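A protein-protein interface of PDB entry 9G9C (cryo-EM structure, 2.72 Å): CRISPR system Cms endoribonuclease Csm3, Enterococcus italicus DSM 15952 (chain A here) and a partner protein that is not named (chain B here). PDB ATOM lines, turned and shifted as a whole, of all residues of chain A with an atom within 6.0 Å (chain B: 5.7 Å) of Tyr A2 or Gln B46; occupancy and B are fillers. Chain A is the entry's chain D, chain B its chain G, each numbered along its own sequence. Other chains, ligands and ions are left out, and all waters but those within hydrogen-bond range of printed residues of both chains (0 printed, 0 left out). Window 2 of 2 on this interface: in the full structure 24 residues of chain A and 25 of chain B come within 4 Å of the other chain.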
ATOM      1  N   TYR A   2      -7.377  21.560  22.152  1.00  0.00           N
ATOM      2  CA  TYR A   2      -8.004  20.212  22.125  1.00  0.00           C
ATOM      3  C   TYR A   2      -9.303  20.299  21.349  1.00  0.00           C
ATOM      4  O   TYR A   2     -10.044  21.293  21.505  1.00  0.00           O
ATOM      5  CB  TYR A   2      -8.278  19.739  23.554  1.00  0.00           C
ATOM      6  CG  TYR A   2      -8.327  18.230  23.744  1.00  0.00           C
ATOM      7  CD1 TYR A   2      -7.172  17.515  24.029  1.00  0.00           C
ATOM      8  CD2 TYR A   2      -9.521  17.527  23.652  1.00  0.00           C
ATOM      9  CE1 TYR A   2      -7.200  16.143  24.209  1.00  0.00           C
ATOM     10  CE2 TYR A   2      -9.562  16.155  23.831  1.00  0.00           C
ATOM     11  CZ  TYR A   2      -8.398  15.462  24.110  1.00  0.00           C
ATOM     12  OH  TYR A   2      -8.411  14.111  24.296  1.00  0.00           O
ATOM     13  N   SER A   3      -9.587  19.281  20.536  1.00  0.00           N
ATOM     14  CA  SER A   3     -10.800  19.327  19.736  1.00  0.00           C
ATOM     15  C   SER A   3     -11.614  18.060  19.947  1.00  0.00           C
ATOM     16  O   SER A   3     -11.072  16.987  20.219  1.00  0.00           O
ATOM     17  CB  SER A   3     -10.483  19.500  18.247  1.00  0.00           C
ATOM     18  OG  SER A   3     -11.661  19.765  17.507  1.00  0.00           O
ATOM     19  N   LYS A   4     -12.931  18.236  19.816  1.00  0.00           N
ATOM     20  CA  LYS A   4     -13.860  17.088  19.921  1.00  0.00           C
ATOM     21  C   LYS A   4     -14.685  17.083  18.632  1.00  0.00           C
ATOM     22  O   LYS A   4     -15.257  18.136  18.297  1.00  0.00           O
ATOM     23  CB  LYS A   4     -14.701  17.173  21.198  1.00  0.00           C
ATOM     24  CG  LYS A   4     -13.920  16.921  22.478  1.00  0.00           C
ATOM     25  CD  LYS A   4     -14.695  17.261  23.743  1.00  0.00           C
ATOM     26  CE  LYS A   4     -13.902  16.944  24.965  1.00  0.00           C
ATOM     27  NZ  LYS A   4     -13.685  15.501  25.101  1.00  0.00           N
ATOM     28  N   SER A  93      -5.682   7.928  27.167  1.00  0.00           N
ATOM     29  CA  SER A  93      -7.126   8.105  27.162  1.00  0.00           C
ATOM     30  C   SER A  93      -7.707   7.631  25.838  1.00  0.00           C
ATOM     31  O   SER A  93      -7.086   7.774  24.782  1.00  0.00           O
ATOM     32  CB  SER A  93      -7.485   9.570  27.401  1.00  0.00           C
ATOM     33  OG  SER A  93      -7.115   9.978  28.705  1.00  0.00           O
ATOM     34  N   ARG A  95      -9.568   7.889  22.647  1.00  0.00           N
ATOM     35  CA  ARG A  95     -10.027   8.965  21.775  1.00  0.00           C
ATOM     36  C   ARG A  95     -11.463   8.733  21.328  1.00  0.00           C
ATOM     37  O   ARG A  95     -12.233   9.688  21.174  1.00  0.00           O
ATOM     38  CB  ARG A  95      -9.101   9.093  20.565  1.00  0.00           C
ATOM     39  CG  ARG A  95      -7.695   9.550  20.906  1.00  0.00           C
ATOM     40  CD  ARG A  95      -6.820   9.618  19.667  1.00  0.00           C
ATOM     41  NE  ARG A  95      -5.415   9.819  19.999  1.00  0.00           N
ATOM     42  CZ  ARG A  95      -4.445   9.954  19.104  1.00  0.00           C
ATOM     43  NH1 ARG A  95      -4.694   9.925  17.806  1.00  0.00           N
ATOM     44  NH2 ARG A  95      -3.194  10.119  19.523  1.00  0.00           N
ATOM     45  N   ASN A 155     -11.740  12.400  20.232  1.00  0.00           N
ATOM     46  CA  ASN A 155     -10.931  13.422  20.939  1.00  0.00           C
ATOM     47  C   ASN A 155      -9.606  13.565  20.191  1.00  0.00           C
ATOM     48  O   ASN A 155      -8.899  12.550  20.045  1.00  0.00           O
ATOM     49  CB  ASN A 155     -10.762  13.040  22.405  1.00  0.00           C
ATOM     50  CG  ASN A 155     -12.066  12.618  23.036  1.00  0.00           C
ATOM     51  OD1 ASN A 155     -12.997  13.424  23.142  1.00  0.00           O
ATOM     52  ND2 ASN A 155     -12.152  11.368  23.463  1.00  0.00           N
ATOM     53  N   VAL A 156      -9.287  14.775  19.739  1.00  0.00           N
ATOM     54  CA  VAL A 156      -8.079  15.035  18.957  1.00  0.00           C
ATOM     55  C   VAL A 156      -6.948  15.233  19.962  1.00  0.00           C
ATOM     56  O   VAL A 156      -6.640  16.351  20.377  1.00  0.00           O
ATOM     57  CB  VAL A 156      -8.251  16.233  18.026  1.00  0.00           C
ATOM     58  CG1 VAL A 156      -7.003  16.448  17.190  1.00  0.00           C
ATOM     59  CG2 VAL A 156      -9.468  16.038  17.129  1.00  0.00           C
ATOM     60  N   GLU A 157      -6.326  14.123  20.365  1.00  0.00           N
ATOM     61  CA  GLU A 157      -5.151  14.212  21.223  1.00  0.00           C
ATOM     62  C   GLU A 157      -3.937  14.704  20.451  1.00  0.00           C
ATOM     63  O   GLU A 157      -3.031  15.308  21.035  1.00  0.00           O
ATOM     64  CB  GLU A 157      -4.855  12.854  21.860  1.00  0.00           C
ATOM     65  CG  GLU A 157      -5.980  12.307  22.715  1.00  0.00           C
ATOM     66  CD  GLU A 157      -5.637  10.968  23.338  1.00  0.00           C
ATOM     67  OE1 GLU A 157      -4.559  10.421  23.027  1.00  0.00           O
ATOM     68  OE2 GLU A 157      -6.447  10.462  24.141  1.00  0.00           O
ATOM     69  N   VAL A 203     -16.246  20.629  19.493  1.00  0.00           N
ATOM     70  CA  VAL A 203     -15.342  21.403  20.395  1.00  0.00           C
ATOM     71  C   VAL A 203     -14.064  21.771  19.630  1.00  0.00           C
ATOM     72  O   VAL A 203     -13.463  20.863  19.030  1.00  0.00           O
ATOM     73  CB  VAL A 203     -15.012  20.637  21.693  1.00  0.00           C
ATOM     74  CG1 VAL A 203     -13.819  21.227  22.434  1.00  0.00           C
ATOM     75  CG2 VAL A 203     -16.219  20.527  22.617  1.00  0.00           C
ATOM     76  N   GLY A 204     -13.701  23.054  19.615  1.00  0.00           N
ATOM     77  CA  GLY A 204     -12.469  23.501  18.996  1.00  0.00           C
ATOM     78  C   GLY A 204     -12.693  24.107  17.624  1.00  0.00           C
ATOM     79  O   GLY A 204     -13.817  24.245  17.131  1.00  0.00           O
ATOM     80  N   ASP A 205     -11.575  24.478  17.005  1.00  0.00           N
ATOM     81  CA  ASP A 205     -11.565  25.077  15.677  1.00  0.00           C
ATOM     82  C   ASP A 205     -11.082  24.111  14.603  1.00  0.00           C
ATOM     83  O   ASP A 205     -10.805  24.541  13.478  1.00  0.00           O
ATOM     84  CB  ASP A 205     -10.699  26.340  15.675  1.00  0.00           C
ATOM     85  CG  ASP A 205      -9.274  26.071  16.118  1.00  0.00           C
ATOM     86  OD1 ASP A 205      -9.087  25.494  17.208  1.00  0.00           O
ATOM     87  OD2 ASP A 205      -8.340  26.435  15.373  1.00  0.00           O
ATOM     88  N   ILE B  41     -11.430  20.095  36.213  1.00  0.00           N
ATOM     89  CA  ILE B  41      -9.955  20.307  36.164  1.00  0.00           C
ATOM     90  C   ILE B  41      -9.428  19.540  34.945  1.00  0.00           C
ATOM     91  O   ILE B  41      -8.712  20.147  34.126  1.00  0.00           O
ATOM     92  CB  ILE B  41      -9.281  19.848  37.470  1.00  0.00           C
ATOM     93  CG1 ILE B  41      -9.692  20.720  38.653  1.00  0.00           C
ATOM     94  CG2 ILE B  41      -7.760  19.798  37.321  1.00  0.00           C
ATOM     95  CD1 ILE B  41      -9.059  22.098  38.658  1.00  0.00           C
ATOM     96  N   ILE B  42      -9.730  18.240  34.864  1.00  0.00           N
ATOM     97  CA  ILE B  42      -9.240  17.388  33.739  1.00  0.00           C
ATOM     98  C   ILE B  42      -9.595  18.073  32.411  1.00  0.00           C
ATOM     99  O   ILE B  42      -8.721  18.125  31.523  1.00  0.00           O
ATOM    100  CB  ILE B  42      -9.831  15.970  33.846  1.00  0.00           C
ATOM    101  CG1 ILE B  42      -9.195  15.197  34.997  1.00  0.00           C
ATOM    102  CG2 ILE B  42      -9.712  15.211  32.525  1.00  0.00           C
ATOM    103  CD1 ILE B  42      -9.826  13.845  35.262  1.00  0.00           C
ATOM    104  N   GLU B  43     -10.815  18.601  32.301  1.00  0.00           N
ATOM    105  CA  GLU B  43     -11.252  19.290  31.063  1.00  0.00           C
ATOM    106  C   GLU B  43     -10.378  20.529  30.847  1.00  0.00           C
ATOM    107  O   GLU B  43      -9.826  20.677  29.745  1.00  0.00           O
ATOM    108  CB  GLU B  43     -12.715  19.715  31.158  1.00  0.00           C
ATOM    109  CG  GLU B  43     -13.391  19.835  29.798  1.00  0.00           C
ATOM    110  CD  GLU B  43     -13.343  18.522  29.043  1.00  0.00           C
ATOM    111  OE1 GLU B  43     -13.865  17.525  29.581  1.00  0.00           O
ATOM    112  OE2 GLU B  43     -12.785  18.492  27.926  1.00  0.00           O
ATOM    113  N   ALA B  44     -10.269  21.386  31.863  1.00  0.00           N
ATOM    114  CA  ALA B  44      -9.484  22.606  31.713  1.00  0.00           C
ATOM    115  C   ALA B  44      -8.058  22.294  31.286  1.00  0.00           C
ATOM    116  O   ALA B  44      -7.480  23.005  30.457  1.00  0.00           O
ATOM    117  CB  ALA B  44      -9.493  23.402  33.018  1.00  0.00           C
ATOM    118  N   LEU B  45      -7.470  21.238  31.850  1.00  0.00           N
ATOM    119  CA  LEU B  45      -6.131  20.833  31.440  1.00  0.00           C
ATOM    120  C   LEU B  45      -6.108  20.406  29.978  1.00  0.00           C
ATOM    121  O   LEU B  45      -5.169  20.733  29.244  1.00  0.00           O
ATOM    122  CB  LEU B  45      -5.631  19.705  32.339  1.00  0.00           C
ATOM    123  CG  LEU B  45      -5.286  20.119  33.767  1.00  0.00           C
ATOM    124  CD1 LEU B  45      -5.387  18.924  34.682  1.00  0.00           C
ATOM    125  CD2 LEU B  45      -3.893  20.719  33.823  1.00  0.00           C
ATOM    126  N   GLN B  46      -7.144  19.696  29.530  1.00  0.00           N
ATOM    127  CA  GLN B  46      -7.217  19.309  28.098  1.00  0.00           C
ATOM    128  C   GLN B  46      -7.343  20.574  27.242  1.00  0.00           C
ATOM    129  O   GLN B  46      -6.616  20.677  26.234  1.00  0.00           O
ATOM    130  CB  GLN B  46      -8.414  18.409  27.803  1.00  0.00           C
ATOM    131  CG  GLN B  46      -8.283  16.988  28.336  1.00  0.00           C
ATOM    132  CD  GLN B  46      -9.465  16.121  27.968  1.00  0.00           C
ATOM    133  OE1 GLN B  46     -10.406  16.566  27.302  1.00  0.00           O
ATOM    134  NE2 GLN B  46      -9.425  14.869  28.399  1.00  0.00           N
ATOM    135  N   GLN B  47      -8.217  21.501  27.634  1.00  0.00           N
ATOM    136  CA  GLN B  47      -8.465  22.705  26.800  1.00  0.00           C
ATOM    137  C   GLN B  47      -7.363  23.755  27.017  1.00  0.00           C
ATOM    138  O   GLN B  47      -7.470  24.833  26.396  1.00  0.00           O
ATOM    139  CB  GLN B  47      -9.851  23.272  27.111  1.00  0.00           C
ATOM    140  CG  GLN B  47     -10.978  22.246  27.061  1.00  0.00           C
ATOM    141  CD  GLN B  47     -11.022  21.449  25.775  1.00  0.00           C
ATOM    142  OE1 GLN B  47     -11.114  22.003  24.674  1.00  0.00           O
ATOM    143  NE2 GLN B  47     -10.956  20.132  25.904  1.00  0.00           N
ATOM    144  N   GLN B  48      -6.353  23.457  27.842  1.00  0.00           N
ATOM    145  CA  GLN B  48      -5.248  24.385  28.085  1.00  0.00           C
ATOM    146  C   GLN B  48      -5.756  25.724  28.624  1.00  0.00           C
ATOM    147  O   GLN B  48      -5.545  26.787  28.040  1.00  0.00           O
ATOM    148  CB  GLN B  48      -4.406  24.584  26.820  1.00  0.00           C
ATOM    149  CG  GLN B  48      -3.373  23.498  26.585  1.00  0.00           C
ATOM    150  CD  GLN B  48      -2.357  23.884  25.531  1.00  0.00           C
ATOM    151  OE1 GLN B  48      -2.708  24.420  24.480  1.00  0.00           O
ATOM    152  NE2 GLN B  48      -1.087  23.615  25.807  1.00  0.00           N
ATOM    153  N   SER B 186     -17.242  14.871  26.834  1.00  0.00           N
ATOM    154  CA  SER B 186     -16.368  14.012  27.681  1.00  0.00           C
ATOM    155  C   SER B 186     -17.214  13.043  28.511  1.00  0.00           C
ATOM    156  O   SER B 186     -16.806  11.873  28.648  1.00  0.00           O
ATOM    157  CB  SER B 186     -15.501  14.841  28.581  1.00  0.00           C
ATOM    158  OG  SER B 186     -14.662  15.709  27.834  1.00  0.00           O
ATOM    159  N   ARG B 192     -17.263   6.128  31.394  1.00  0.00           N
ATOM    160  CA  ARG B 192     -17.434   7.162  30.339  1.00  0.00           C
ATOM    161  C   ARG B 192     -16.394   6.774  29.281  1.00  0.00           C
ATOM    162  O   ARG B 192     -15.340   6.250  29.717  1.00  0.00           O
ATOM    163  CB  ARG B 192     -17.251   8.590  30.859  1.00  0.00           C
ATOM    164  CG  ARG B 192     -15.903   8.837  31.516  1.00  0.00           C
ATOM    165  CD  ARG B 192     -15.609  10.315  31.624  1.00  0.00           C
ATOM    166  NE  ARG B 192     -14.166  10.525  31.772  1.00  0.00           N
ATOM    167  CZ  ARG B 192     -13.425  11.188  30.900  1.00  0.00           C
ATOM    168  NH1 ARG B 192     -13.963  11.617  29.772  1.00  0.00           N
ATOM    169  NH2 ARG B 192     -12.152  11.421  31.159  1.00  0.00           N
ATOM    170  N   LYS B 254      -2.700  10.558  32.682  1.00  0.00           N
ATOM    171  CA  LYS B 254      -1.633   9.893  31.953  1.00  0.00           C
ATOM    172  C   LYS B 254      -0.245  10.263  32.456  1.00  0.00           C
ATOM    173  O   LYS B 254       0.732   9.618  32.061  1.00  0.00           O
ATOM    174  CB  LYS B 254      -1.719  10.224  30.459  1.00  0.00           C
ATOM    175  CG  LYS B 254      -3.125  10.452  29.935  1.00  0.00           C
ATOM    176  CD  LYS B 254      -3.086  10.889  28.478  1.00  0.00           C
ATOM    177  CE  LYS B 254      -4.404  11.502  28.036  1.00  0.00           C
ATOM    178  NZ  LYS B 254      -4.696  12.780  28.742  1.00  0.00           N
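Among the printed residues, pairs that only touch across the chains: Tyr A2 with Gln B46, Lys A4 with Glu B43, Ser A93 with Lys B254 and Val A203 with Gln B47.
OE1 of Gln B47 lies close to O of Tyr A2, at 3.4 Å.
The side-chain amino group (NZ) of Lys A4 sits at hydrogen-bond distance from the side-chain hydroxyl (OG) of Ser B186 (2.9 Å).
The backbone carbonyl oxygen (O) of Val A203 is in hydrogen-bond range of the side-chain hydroxyl (OG) of Ser A3 (2.6 Å).
The side-chain amino group (NZ) of Lys A4 sits at hydrogen-bond distance from the side-chain amide oxygen (OD1) of Asn A155 (2.9 Å).
N of Lys A4 lies within hydrogen-bond range of O of Val A203, at 2.8 Å.
The side-chain amide oxygen (OE1) of Gln B46 lies close to the side-chain carboxylate (OE2) of Glu B43 (3.1 Å).
OE2 of Glu B43 sits at hydrogen-bond distance from NE2 of Gln B47 (3.2 Å).
NH1 of Arg B192 sits at hydrogen-bond distance from O of Ser B186, at 3.1 Å.
Printed residues of chain B within 4 Å of Lys A4: Glu B43 (3.5 Å) and Ser B186 (2.9 Å).
Printed residues of chain B within 4 Å of Val A203: Gln B47.
Of the printed residues of chain A, Glu B43 touches Lys A4 (3.5 Å).
Of chain A, only Tyr A2 (3.3 Å) comes within 4 Å of Gln B46.
Of the printed residues of chain A, Lys B254 touches Ser A93.
The nearest residue of chain B that does not touch Tyr A2 is Glu B43 (5.5 Å).
The nearest residue of chain A that does not touch Gln B46 is Lys A4 (4.1 Å).
Printed residues of chain B that touch a printed residue of chain A: Glu B43, Gln B46, Gln B47, Ser B186 and Lys B254.
Hydrophobic or aromatic side chains of chain A that line the printed part of chain B: Tyr A2 and Val A203.
Among the printed residues, no Asp or Glu carboxylate lies within 4 Å of a Lys or Arg side-chain nitrogen of the other chain.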
